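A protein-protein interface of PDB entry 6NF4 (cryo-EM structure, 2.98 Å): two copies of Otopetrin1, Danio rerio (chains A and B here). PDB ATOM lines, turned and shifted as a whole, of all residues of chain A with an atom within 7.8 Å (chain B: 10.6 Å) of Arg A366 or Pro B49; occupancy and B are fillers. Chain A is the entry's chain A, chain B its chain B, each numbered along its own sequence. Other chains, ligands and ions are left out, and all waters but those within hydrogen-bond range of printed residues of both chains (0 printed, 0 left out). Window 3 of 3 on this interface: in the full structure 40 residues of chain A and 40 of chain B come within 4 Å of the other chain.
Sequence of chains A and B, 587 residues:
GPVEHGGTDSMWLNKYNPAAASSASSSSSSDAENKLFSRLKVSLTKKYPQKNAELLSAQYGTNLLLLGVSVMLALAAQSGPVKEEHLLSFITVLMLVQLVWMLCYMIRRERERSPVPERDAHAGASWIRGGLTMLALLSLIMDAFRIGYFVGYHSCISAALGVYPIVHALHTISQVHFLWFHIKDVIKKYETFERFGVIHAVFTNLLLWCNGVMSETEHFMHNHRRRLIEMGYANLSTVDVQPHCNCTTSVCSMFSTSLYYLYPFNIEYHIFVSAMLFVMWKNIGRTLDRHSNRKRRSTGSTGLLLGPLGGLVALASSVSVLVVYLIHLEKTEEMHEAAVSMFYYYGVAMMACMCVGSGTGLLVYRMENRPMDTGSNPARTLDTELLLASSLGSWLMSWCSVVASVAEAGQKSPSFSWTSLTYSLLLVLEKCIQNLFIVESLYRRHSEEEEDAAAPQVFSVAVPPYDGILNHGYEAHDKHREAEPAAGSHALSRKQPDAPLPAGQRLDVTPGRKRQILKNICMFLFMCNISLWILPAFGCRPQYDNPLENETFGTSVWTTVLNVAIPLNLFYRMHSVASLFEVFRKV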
ATOM      1  N   GLY A 359      34.268  11.398   6.338  1.00  0.00           N
ATOM      2  CA  GLY A 359      33.052  12.186   6.226  1.00  0.00           C
ATOM      3  C   GLY A 359      31.821  11.338   5.973  1.00  0.00           C
ATOM      4  O   GLY A 359      30.742  11.620   6.496  1.00  0.00           O
ATOM      5  N   THR A 360      31.966  10.292   5.154  1.00  0.00           N
ATOM      6  CA  THR A 360      30.857   9.377   4.901  1.00  0.00           C
ATOM      7  C   THR A 360      30.446   8.640   6.170  1.00  0.00           C
ATOM      8  O   THR A 360      29.249   8.471   6.441  1.00  0.00           O
ATOM      9  CB  THR A 360      31.252   8.398   3.803  1.00  0.00           C
ATOM     10  OG1 THR A 360      31.602   9.135   2.632  1.00  0.00           O
ATOM     11  CG2 THR A 360      30.109   7.471   3.463  1.00  0.00           C
ATOM     12  N   GLY A 361      31.431   8.210   6.965  1.00  0.00           N
ATOM     13  CA  GLY A 361      31.136   7.635   8.272  1.00  0.00           C
ATOM     14  C   GLY A 361      30.391   8.587   9.189  1.00  0.00           C
ATOM     15  O   GLY A 361      29.421   8.203   9.852  1.00  0.00           O
ATOM     16  N   LEU A 362      30.826   9.852   9.223  1.00  0.00           N
ATOM     17  CA  LEU A 362      30.160  10.846  10.062  1.00  0.00           C
ATOM     18  C   LEU A 362      28.731  11.121   9.605  1.00  0.00           C
ATOM     19  O   LEU A 362      27.840  11.308  10.436  1.00  0.00           O
ATOM     20  CB  LEU A 362      30.960  12.144  10.095  1.00  0.00           C
ATOM     21  CG  LEU A 362      32.210  12.098  10.962  1.00  0.00           C
ATOM     22  CD1 LEU A 362      33.014  13.359  10.807  1.00  0.00           C
ATOM     23  CD2 LEU A 362      31.817  11.898  12.399  1.00  0.00           C
ATOM     24  N   LEU A 363      28.486  11.133   8.293  1.00  0.00           N
ATOM     25  CA  LEU A 363      27.124  11.360   7.807  1.00  0.00           C
ATOM     26  C   LEU A 363      26.216  10.165   8.069  1.00  0.00           C
ATOM     27  O   LEU A 363      25.016  10.339   8.328  1.00  0.00           O
ATOM     28  CB  LEU A 363      27.137  11.722   6.326  1.00  0.00           C
ATOM     29  CG  LEU A 363      27.148  13.214   5.974  1.00  0.00           C
ATOM     30  CD1 LEU A 363      28.406  13.929   6.413  1.00  0.00           C
ATOM     31  CD2 LEU A 363      26.952  13.383   4.477  1.00  0.00           C
ATOM     32  N   VAL A 364      26.762   8.945   8.007  1.00  0.00           N
ATOM     33  CA  VAL A 364      25.990   7.766   8.403  1.00  0.00           C
ATOM     34  C   VAL A 364      25.636   7.837   9.885  1.00  0.00           C
ATOM     35  O   VAL A 364      24.523   7.483  10.294  1.00  0.00           O
ATOM     36  CB  VAL A 364      26.759   6.480   8.044  1.00  0.00           C
ATOM     37  CG1 VAL A 364      26.126   5.249   8.661  1.00  0.00           C
ATOM     38  CG2 VAL A 364      26.796   6.312   6.543  1.00  0.00           C
ATOM     39  N   TYR A 365      26.560   8.341  10.705  1.00  0.00           N
ATOM     40  CA  TYR A 365      26.248   8.567  12.116  1.00  0.00           C
ATOM     41  C   TYR A 365      25.194   9.652  12.314  1.00  0.00           C
ATOM     42  O   TYR A 365      24.360   9.546  13.218  1.00  0.00           O
ATOM     43  CB  TYR A 365      27.512   8.938  12.882  1.00  0.00           C
ATOM     44  CG  TYR A 365      28.436   7.786  13.140  1.00  0.00           C
ATOM     45  CD1 TYR A 365      27.979   6.478  13.112  1.00  0.00           C
ATOM     46  CD2 TYR A 365      29.768   8.009  13.415  1.00  0.00           C
ATOM     47  CE1 TYR A 365      28.831   5.427  13.352  1.00  0.00           C
ATOM     48  CE2 TYR A 365      30.617   6.977  13.652  1.00  0.00           C
ATOM     49  CZ  TYR A 365      30.151   5.686  13.621  1.00  0.00           C
ATOM     50  OH  TYR A 365      31.021   4.653  13.863  1.00  0.00           O
ATOM     51  N   ARG A 366      25.224  10.712  11.501  1.00  0.00           N
ATOM     52  CA  ARG A 366      24.281  11.813  11.698  1.00  0.00           C
ATOM     53  C   ARG A 366      22.871  11.434  11.272  1.00  0.00           C
ATOM     54  O   ARG A 366      21.899  11.884  11.885  1.00  0.00           O
ATOM     55  CB  ARG A 366      24.720  13.070  10.946  1.00  0.00           C
ATOM     56  CG  ARG A 366      25.982  13.758  11.455  1.00  0.00           C
ATOM     57  CD  ARG A 366      25.781  14.621  12.705  1.00  0.00           C
ATOM     58  NE  ARG A 366      25.686  13.853  13.941  1.00  0.00           N
ATOM     59  CZ  ARG A 366      26.717  13.311  14.579  1.00  0.00           C
ATOM     60  NH1 ARG A 366      27.950  13.447  14.113  1.00  0.00           N
ATOM     61  NH2 ARG A 366      26.514  12.627  15.694  1.00  0.00           N
ATOM     62  N   MET A 367      22.736  10.646  10.203  1.00  0.00           N
ATOM     63  CA  MET A 367      21.402  10.257   9.753  1.00  0.00           C
ATOM     64  C   MET A 367      20.721   9.321  10.745  1.00  0.00           C
ATOM     65  O   MET A 367      19.503   9.396  10.938  1.00  0.00           O
ATOM     66  CB  MET A 367      21.472   9.624   8.367  1.00  0.00           C
ATOM     67  CG  MET A 367      21.765  10.621   7.263  1.00  0.00           C
ATOM     68  SD  MET A 367      21.356   9.992   5.628  1.00  0.00           S
ATOM     69  CE  MET A 367      22.240   8.439   5.640  1.00  0.00           C
ATOM     70  N   GLU A 368      21.482   8.442  11.387  1.00  0.00           N
ATOM     71  CA  GLU A 368      20.931   7.583  12.431  1.00  0.00           C
ATOM     72  C   GLU A 368      20.921   8.349  13.750  1.00  0.00           C
ATOM     73  O   GLU A 368      21.962   8.492  14.398  1.00  0.00           O
ATOM     74  CB  GLU A 368      21.747   6.299  12.549  1.00  0.00           C
ATOM     75  CG  GLU A 368      21.212   5.318  13.583  1.00  0.00           C
ATOM     76  CD  GLU A 368      22.028   4.042  13.662  1.00  0.00           C
ATOM     77  OE1 GLU A 368      23.027   3.924  12.922  1.00  0.00           O
ATOM     78  OE2 GLU A 368      21.674   3.157  14.467  1.00  0.00           O
ATOM     79  N   ASN A 369      19.749   8.821  14.168  1.00  0.00           N
ATOM     80  CA  ASN A 369      19.640   9.597  15.397  1.00  0.00           C
ATOM     81  C   ASN A 369      19.662   8.691  16.618  1.00  0.00           C
ATOM     82  O   ASN A 369      19.078   7.604  16.614  1.00  0.00           O
ATOM     83  CB  ASN A 369      18.370  10.445  15.393  1.00  0.00           C
ATOM     84  CG  ASN A 369      18.500  11.679  14.528  1.00  0.00           C
ATOM     85  OD1 ASN A 369      19.530  12.352  14.541  1.00  0.00           O
ATOM     86  ND2 ASN A 369      17.456  11.985  13.769  1.00  0.00           N
ATOM     87  N   ARG A 370      20.341   9.146  17.664  1.00  0.00           N
ATOM     88  CA  ARG A 370      20.540   8.419  18.898  1.00  0.00           C
ATOM     89  C   ARG A 370      20.329   9.373  20.067  1.00  0.00           C
ATOM     90  O   ARG A 370      20.502  10.588  19.915  1.00  0.00           O
ATOM     91  CB  ARG A 370      21.959   7.837  18.967  1.00  0.00           C
ATOM     92  CG  ARG A 370      22.217   6.603  18.133  1.00  0.00           C
ATOM     93  CD  ARG A 370      21.677   5.353  18.780  1.00  0.00           C
ATOM     94  NE  ARG A 370      22.246   4.169  18.147  1.00  0.00           N
ATOM     95  CZ  ARG A 370      22.860   3.193  18.807  1.00  0.00           C
ATOM     96  NH1 ARG A 370      22.989   3.262  20.125  1.00  0.00           N
ATOM     97  NH2 ARG A 370      23.355   2.151  18.153  1.00  0.00           N
ATOM     98  N   MET A 372      22.124  10.863  22.234  1.00  0.00           N
ATOM     99  CA  MET A 372      23.567  11.015  22.282  1.00  0.00           C
ATOM    100  C   MET A 372      24.037  11.637  23.597  1.00  0.00           C
ATOM    101  O   MET A 372      23.347  12.452  24.217  1.00  0.00           O
ATOM    102  CB  MET A 372      24.036  11.879  21.107  1.00  0.00           C
ATOM    103  CG  MET A 372      23.796  11.298  19.718  1.00  0.00           C
ATOM    104  SD  MET A 372      24.896   9.915  19.366  1.00  0.00           S
ATOM    105  CE  MET A 372      24.855   9.887  17.573  1.00  0.00           C
ATOM    106  N   ASP A 373      25.230  11.199  24.025  1.00  0.00           N
ATOM    107  CA  ASP A 373      26.125  11.945  24.924  1.00  0.00           C
ATOM    108  C   ASP A 373      25.538  12.195  26.310  1.00  0.00           C
ATOM    109  O   ASP A 373      25.601  13.306  26.840  1.00  0.00           O
ATOM    110  CB  ASP A 373      26.547  13.260  24.282  1.00  0.00           C
ATOM    111  CG  ASP A 373      27.088  13.064  22.893  1.00  0.00           C
ATOM    112  OD1 ASP A 373      27.298  11.897  22.502  1.00  0.00           O
ATOM    113  OD2 ASP A 373      27.313  14.070  22.196  1.00  0.00           O
ATOM    114  N   ARG A 380      36.371   8.695  27.390  1.00  0.00           N
ATOM    115  CA  ARG A 380      36.286   9.485  26.167  1.00  0.00           C
ATOM    116  C   ARG A 380      37.226  10.676  26.217  1.00  0.00           C
ATOM    117  O   ARG A 380      37.909  10.975  25.232  1.00  0.00           O
ATOM    118  CB  ARG A 380      34.845   9.939  25.938  1.00  0.00           C
ATOM    119  CG  ARG A 380      34.580  10.494  24.553  1.00  0.00           C
ATOM    120  CD  ARG A 380      33.093  10.682  24.302  1.00  0.00           C
ATOM    121  NE  ARG A 380      32.817  10.929  22.894  1.00  0.00           N
ATOM    122  CZ  ARG A 380      31.603  11.095  22.381  1.00  0.00           C
ATOM    123  NH1 ARG A 380      31.454  11.321  21.084  1.00  0.00           N
ATOM    124  NH2 ARG A 380      30.535  11.009  23.155  1.00  0.00           N
ATOM    125  N   LEU A 436      37.487  13.132  14.860  1.00  0.00           N
ATOM    126  CA  LEU A 436      36.068  13.226  15.185  1.00  0.00           C
ATOM    127  C   LEU A 436      35.352  11.904  14.927  1.00  0.00           C
ATOM    128  O   LEU A 436      34.541  11.460  15.749  1.00  0.00           O
ATOM    129  CB  LEU A 436      35.448  14.363  14.383  1.00  0.00           C
ATOM    130  CG  LEU A 436      34.012  14.771  14.651  1.00  0.00           C
ATOM    131  CD1 LEU A 436      33.871  15.189  16.087  1.00  0.00           C
ATOM    132  CD2 LEU A 436      33.663  15.915  13.735  1.00  0.00           C
ATOM    133  N   GLU A 440      33.770   9.607  17.977  1.00  0.00           N
ATOM    134  CA  GLU A 440      32.341   9.300  17.962  1.00  0.00           C
ATOM    135  C   GLU A 440      32.085   7.803  17.817  1.00  0.00           C
ATOM    136  O   GLU A 440      31.143   7.272  18.413  1.00  0.00           O
ATOM    137  CB  GLU A 440      31.635  10.077  16.855  1.00  0.00           C
ATOM    138  CG  GLU A 440      30.127   9.925  16.895  1.00  0.00           C
ATOM    139  CD  GLU A 440      29.413  10.907  16.013  1.00  0.00           C
ATOM    140  OE1 GLU A 440      29.688  10.920  14.800  1.00  0.00           O
ATOM    141  OE2 GLU A 440      28.570  11.665  16.531  1.00  0.00           O
ATOM    142  N   ARG A 444      29.481   5.114  21.142  1.00  0.00           N
ATOM    143  CA  ARG A 444      28.059   5.107  20.826  1.00  0.00           C
ATOM    144  C   ARG A 444      27.301   4.148  21.734  1.00  0.00           C
ATOM    145  O   ARG A 444      27.006   3.017  21.351  1.00  0.00           O
ATOM    146  CB  ARG A 444      27.833   4.730  19.367  1.00  0.00           C
ATOM    147  CG  ARG A 444      28.218   5.818  18.404  1.00  0.00           C
ATOM    148  CD  ARG A 444      28.247   5.321  16.975  1.00  0.00           C
ATOM    149  NE  ARG A 444      26.941   4.877  16.509  1.00  0.00           N
ATOM    150  CZ  ARG A 444      25.999   5.688  16.040  1.00  0.00           C
ATOM    151  NH1 ARG A 444      26.212   6.993  15.973  1.00  0.00           N
ATOM    152  NH2 ARG A 444      24.841   5.191  15.636  1.00  0.00           N
ATOM    153  N   LYS B  47      19.767  19.265  17.864  1.00  0.00           N
ATOM    154  CA  LYS B  47      20.175  19.364  16.470  1.00  0.00           C
ATOM    155  C   LYS B  47      21.563  18.775  16.266  1.00  0.00           C
ATOM    156  O   LYS B  47      21.802  18.043  15.307  1.00  0.00           O
ATOM    157  CB  LYS B  47      20.153  20.821  16.006  1.00  0.00           C
ATOM    158  CG  LYS B  47      20.577  21.007  14.561  1.00  0.00           C
ATOM    159  CD  LYS B  47      20.461  22.451  14.116  1.00  0.00           C
ATOM    160  CE  LYS B  47      20.931  22.607  12.678  1.00  0.00           C
ATOM    161  NZ  LYS B  47      20.845  24.018  12.218  1.00  0.00           N
ATOM    162  N   TYR B  48      22.474  19.085  17.188  1.00  0.00           N
ATOM    163  CA  TYR B  48      23.858  18.688  17.049  1.00  0.00           C
ATOM    164  C   TYR B  48      24.372  18.236  18.408  1.00  0.00           C
ATOM    165  O   TYR B  48      24.080  18.892  19.419  1.00  0.00           O
ATOM    166  CB  TYR B  48      24.715  19.835  16.513  1.00  0.00           C
ATOM    167  CG  TYR B  48      26.046  19.392  15.967  1.00  0.00           C
ATOM    168  CD1 TYR B  48      26.147  18.874  14.684  1.00  0.00           C
ATOM    169  CD2 TYR B  48      27.200  19.492  16.727  1.00  0.00           C
ATOM    170  CE1 TYR B  48      27.359  18.468  14.176  1.00  0.00           C
ATOM    171  CE2 TYR B  48      28.420  19.089  16.224  1.00  0.00           C
ATOM    172  CZ  TYR B  48      28.490  18.576  14.949  1.00  0.00           C
ATOM    173  OH  TYR B  48      29.692  18.166  14.433  1.00  0.00           O
ATOM    174  N   PRO B  49      25.110  17.129  18.468  1.00  0.00           N
ATOM    175  CA  PRO B  49      25.544  16.593  19.761  1.00  0.00           C
ATOM    176  C   PRO B  49      26.606  17.456  20.422  1.00  0.00           C
ATOM    177  O   PRO B  49      27.326  18.210  19.765  1.00  0.00           O
ATOM    178  CB  PRO B  49      26.099  15.212  19.397  1.00  0.00           C
ATOM    179  CG  PRO B  49      26.447  15.311  17.974  1.00  0.00           C
ATOM    180  CD  PRO B  49      25.444  16.221  17.362  1.00  0.00           C
ATOM    181  N   GLN B  50      26.689  17.348  21.748  1.00  0.00           N
ATOM    182  CA  GLN B  50      27.557  18.240  22.510  1.00  0.00           C
ATOM    183  C   GLN B  50      29.005  17.777  22.550  1.00  0.00           C
ATOM    184  O   GLN B  50      29.908  18.615  22.558  1.00  0.00           O
ATOM    185  CB  GLN B  50      27.035  18.403  23.934  1.00  0.00           C
ATOM    186  CG  GLN B  50      25.650  19.000  23.995  1.00  0.00           C
ATOM    187  CD  GLN B  50      25.558  20.341  23.289  1.00  0.00           C
ATOM    188  OE1 GLN B  50      24.687  20.548  22.446  1.00  0.00           O
ATOM    189  NE2 GLN B  50      26.453  21.259  23.638  1.00  0.00           N
ATOM    190  N   LYS B  51      29.251  16.469  22.598  1.00  0.00           N
ATOM    191  CA  LYS B  51      30.623  15.968  22.616  1.00  0.00           C
ATOM    192  C   LYS B  51      31.342  16.250  21.304  1.00  0.00           C
ATOM    193  O   LYS B  51      32.536  16.579  21.301  1.00  0.00           O
ATOM    194  CB  LYS B  51      30.623  14.471  22.911  1.00  0.00           C
ATOM    195  CG  LYS B  51      30.199  14.114  24.320  1.00  0.00           C
ATOM    196  CD  LYS B  51      31.256  14.440  25.353  1.00  0.00           C
ATOM    197  CE  LYS B  51      30.682  14.341  26.759  1.00  0.00           C
ATOM    198  NZ  LYS B  51      31.635  13.739  27.725  1.00  0.00           N
ATOM    199  N   ASN B  52      30.618  16.215  20.190  1.00  0.00           N
ATOM    200  CA  ASN B  52      31.220  16.584  18.922  1.00  0.00           C
ATOM    201  C   ASN B  52      31.436  18.084  18.832  1.00  0.00           C
ATOM    202  O   ASN B  52      32.416  18.525  18.225  1.00  0.00           O
ATOM    203  CB  ASN B  52      30.346  16.110  17.766  1.00  0.00           C
ATOM    204  CG  ASN B  52      30.306  14.613  17.660  1.00  0.00           C
ATOM    205  OD1 ASN B  52      31.048  13.915  18.345  1.00  0.00           O
ATOM    206  ND2 ASN B  52      29.454  14.105  16.783  1.00  0.00           N
ATOM    207  N   ALA B  53      30.544  18.866  19.445  1.00  0.00           N
ATOM    208  CA  ALA B  53      30.726  20.312  19.502  1.00  0.00           C
ATOM    209  C   ALA B  53      31.969  20.682  20.292  1.00  0.00           C
ATOM    210  O   ALA B  53      32.765  21.518  19.848  1.00  0.00           O
ATOM    211  CB  ALA B  53      29.499  20.977  20.116  1.00  0.00           C
ATOM    212  N   GLU B  54      32.174  20.049  21.449  1.00  0.00           N
ATOM    213  CA  GLU B  54      33.338  20.387  22.259  1.00  0.00           C
ATOM    214  C   GLU B  54      34.626  19.870  21.626  1.00  0.00           C
ATOM    215  O   GLU B  54      35.669  20.524  21.715  1.00  0.00           O
ATOM    216  CB  GLU B  54      33.167  19.900  23.699  1.00  0.00           C
ATOM    217  CG  GLU B  54      33.237  18.424  23.948  1.00  0.00           C
ATOM    218  CD  GLU B  54      33.193  18.107  25.431  1.00  0.00           C
ATOM    219  OE1 GLU B  54      32.159  17.595  25.896  1.00  0.00           O
ATOM    220  OE2 GLU B  54      34.191  18.376  26.127  1.00  0.00           O
ATOM    221  N   LEU B  55      34.569  18.728  20.935  1.00  0.00           N
ATOM    222  CA  LEU B  55      35.763  18.237  20.249  1.00  0.00           C
ATOM    223  C   LEU B  55      36.122  19.106  19.044  1.00  0.00           C
ATOM    224  O   LEU B  55      37.302  19.400  18.820  1.00  0.00           O
ATOM    225  CB  LEU B  55      35.572  16.781  19.841  1.00  0.00           C
ATOM    226  CG  LEU B  55      36.716  16.124  19.074  1.00  0.00           C
ATOM    227  CD1 LEU B  55      38.016  16.232  19.819  1.00  0.00           C
ATOM    228  CD2 LEU B  55      36.390  14.681  18.839  1.00  0.00           C
ATOM    229  N   LEU B  56      35.125  19.534  18.261  1.00  0.00           N
ATOM    230  CA  LEU B  56      35.394  20.446  17.150  1.00  0.00           C
ATOM    231  C   LEU B  56      35.916  21.787  17.632  1.00  0.00           C
ATOM    232  O   LEU B  56      36.802  22.373  17.003  1.00  0.00           O
ATOM    233  CB  LEU B  56      34.144  20.668  16.312  1.00  0.00           C
ATOM    234  CG  LEU B  56      33.798  19.635  15.260  1.00  0.00           C
ATOM    235  CD1 LEU B  56      32.441  19.956  14.713  1.00  0.00           C
ATOM    236  CD2 LEU B  56      34.831  19.686  14.165  1.00  0.00           C
ATOM    237  N   SER B  57      35.375  22.293  18.743  1.00  0.00           N
ATOM    238  CA  SER B  57      35.854  23.559  19.277  1.00  0.00           C
ATOM    239  C   SER B  57      37.274  23.432  19.805  1.00  0.00           C
ATOM    240  O   SER B  57      38.087  24.345  19.629  1.00  0.00           O
ATOM    241  CB  SER B  57      34.918  24.049  20.370  1.00  0.00           C
ATOM    242  OG  SER B  57      34.966  23.179  21.479  1.00  0.00           O
ATOM    243  N   TYR B 190      24.292  26.040  26.910  1.00  0.00           N
ATOM    244  CA  TYR B 190      25.616  25.792  26.349  1.00  0.00           C
ATOM    245  C   TYR B 190      25.428  25.017  25.051  1.00  0.00           C
ATOM    246  O   TYR B 190      24.905  23.900  25.052  1.00  0.00           O
ATOM    247  CB  TYR B 190      26.531  25.064  27.342  1.00  0.00           C
ATOM    248  CG  TYR B 190      25.983  23.802  27.993  1.00  0.00           C
ATOM    249  CD1 TYR B 190      25.201  23.869  29.146  1.00  0.00           C
ATOM    250  CD2 TYR B 190      26.302  22.542  27.496  1.00  0.00           C
ATOM    251  CE1 TYR B 190      24.716  22.720  29.751  1.00  0.00           C
ATOM    252  CE2 TYR B 190      25.821  21.390  28.094  1.00  0.00           C
ATOM    253  CZ  TYR B 190      25.033  21.486  29.220  1.00  0.00           C
ATOM    254  OH  TYR B 190      24.561  20.338  29.811  1.00  0.00           O
ATOM    255  N   GLU B 191      25.800  25.641  23.940  1.00  0.00           N
ATOM    256  CA  GLU B 191      25.644  25.072  22.612  1.00  0.00           C
ATOM    257  C   GLU B 191      26.926  25.289  21.828  1.00  0.00           C
ATOM    258  O   GLU B 191      27.964  25.641  22.387  1.00  0.00           O
ATOM    259  CB  GLU B 191      24.444  25.682  21.882  1.00  0.00           C
ATOM    260  CG  GLU B 191      23.158  24.921  22.108  1.00  0.00           C
ATOM    261  CD  GLU B 191      22.019  25.442  21.264  1.00  0.00           C
ATOM    262  OE1 GLU B 191      21.129  24.641  20.913  1.00  0.00           O
ATOM    263  OE2 GLU B 191      22.014  26.650  20.950  1.00  0.00           O
ATOM    264  N   THR B 192      26.844  25.053  20.517  1.00  0.00           N
ATOM    265  CA  THR B 192      28.004  25.202  19.645  1.00  0.00           C
ATOM    266  C   THR B 192      28.470  26.653  19.573  1.00  0.00           C
ATOM    267  O   THR B 192      29.677  26.920  19.494  1.00  0.00           O
ATOM    268  CB  THR B 192      27.649  24.672  18.254  1.00  0.00           C
ATOM    269  OG1 THR B 192      27.127  23.344  18.377  1.00  0.00           O
ATOM    270  CG2 THR B 192      28.871  24.617  17.357  1.00  0.00           C
ATOM    271  N   PHE B 193      27.526  27.594  19.661  1.00  0.00           N
ATOM    272  CA  PHE B 193      27.826  29.017  19.535  1.00  0.00           C
ATOM    273  C   PHE B 193      28.669  29.510  20.706  1.00  0.00           C
ATOM    274  O   PHE B 193      29.720  30.138  20.517  1.00  0.00           O
ATOM    275  CB  PHE B 193      26.500  29.773  19.426  1.00  0.00           C
ATOM    276  CG  PHE B 193      26.632  31.243  19.175  1.00  0.00           C
ATOM    277  CD1 PHE B 193      27.030  31.718  17.937  1.00  0.00           C
ATOM    278  CD2 PHE B 193      26.284  32.153  20.158  1.00  0.00           C
ATOM    279  CE1 PHE B 193      27.128  33.076  17.701  1.00  0.00           C
ATOM    280  CE2 PHE B 193      26.378  33.510  19.928  1.00  0.00           C
ATOM    281  CZ  PHE B 193      26.799  33.972  18.698  1.00  0.00           C
ATOM    282  N   ARG B 195      30.384  27.592  22.835  1.00  0.00           N
ATOM    283  CA  ARG B 195      31.651  26.863  22.898  1.00  0.00           C
ATOM    284  C   ARG B 195      32.670  27.436  21.926  1.00  0.00           C
ATOM    285  O   ARG B 195      33.845  27.600  22.282  1.00  0.00           O
ATOM    286  CB  ARG B 195      31.432  25.382  22.622  1.00  0.00           C
ATOM    287  CG  ARG B 195      30.779  24.644  23.756  1.00  0.00           C
ATOM    288  CD  ARG B 195      30.649  23.172  23.437  1.00  0.00           C
ATOM    289  NE  ARG B 195      29.877  22.466  24.449  1.00  0.00           N
ATOM    290  CZ  ARG B 195      30.373  22.019  25.595  1.00  0.00           C
ATOM    291  NH1 ARG B 195      31.655  22.196  25.885  1.00  0.00           N
ATOM    292  NH2 ARG B 195      29.584  21.392  26.453  1.00  0.00           N
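No position is printed for both chains.
Of the 11 pairs that touch across the chains among the printed residues, none has its exchanged pair printed and touching as well.
The side-chain carboxylate of Glu A440 is in salt-bridge range of the guanidinium group of Arg A366 (2.4 Å).
OD1 of Asp A373 lies within salt-bridge range of NH2 of Arg A380 (3.4 Å).
The side-chain amide nitrogen (NE2) of Gln B50 sits at hydrogen-bond distance from the backbone carbonyl oxygen (O) of Tyr B190, 3.4 Å away.
NH1 of Arg A366 sits close to ND2 of Asn B52, 3.1 Å away.
The side-chain carboxylate (OD2) of Asp A373 is in hydrogen-bond range of the backbone NH (N) of Gln B50 (3.4 Å).
The side-chain carboxylate (OD2) of Asp A373 lies within hydrogen-bond range of the backbone NH (N) of Lys B51.
The side-chain carboxylate (OE2) of Glu A440 is in hydrogen-bond range of the side-chain amide nitrogen (ND2) of Asn B52 (2.6 Å).
Of the 18 printed residues of chain A, 5 touch a printed residue of chain B.
Printed residues of chain A that touch a printed residue of chain B: Arg A366, Asp A373, Arg A380, Leu A436 and Glu A440.
Of the 16 printed residues of chain B, 6 touch a printed residue of chain A.
Printed residues of chain B that touch a printed residue of chain A: Pro B49, Gln B50, Lys B51, Asn B52, Leu B55 and Leu B56.
Along chain B the printed residues that touch a printed residue of chain A span positions 49 to 56.
Among the printed residues, no Asp or Glu carboxylate lies within 4 Å of a Lys or Arg side-chain nitrogen of the other chain.
Of chain B, only Pro B49 (3.5 Å) and Asn B52 (3.1 Å) come within 4 Å of Arg A366.
Pro B49 touches just these residues of chain A: Arg A366 (3.5 Å) and Asp A373 (3.3 Å).
No residue of chain B comes within 4 Å of Leu A362.
No residue of chain B comes within 4 Å of Met A367.
No residue of chain B comes within 4 Å of Met A372.
Of the printed residues of chain A, Leu B55 touches Leu A436.
Of the printed residues of chain A, Asn B52 touches Arg A366, Arg A380, Leu A436 and Glu A440.
Printed residues of chain B within 4 Å of Glu A440: Asn B52.
Of the printed residues of chain B, Arg A380 touches Lys B51 and Asn B52.
Of the printed residues of chain A, Gln B50 touches Asp A373 (3.4 Å).
Tyr A365 touches none of the printed residues of chain B.
The nearest residue of chain B that does not touch Arg A366 is Tyr B48 (4.4 Å).
NH2 of Arg A366 touches CG of Pro B49 (3.5 Å).
Pro B49 touches Asp A373.
Arg A380 touches Lys B51 (NH2 to CG, 3.3 Å).
NH1 of Arg A380 touches OD1 of Asn B52, 3.8 Å away.
Leu A436 touches Asn B52 (CD1 to OD1, 3.8 Å).
CD2 of Leu B55 touches CD1 of Leu A436, at 3.8 Å.
CD2 of Leu A436 touches CD2 of Leu B56, 3.97 Å away.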
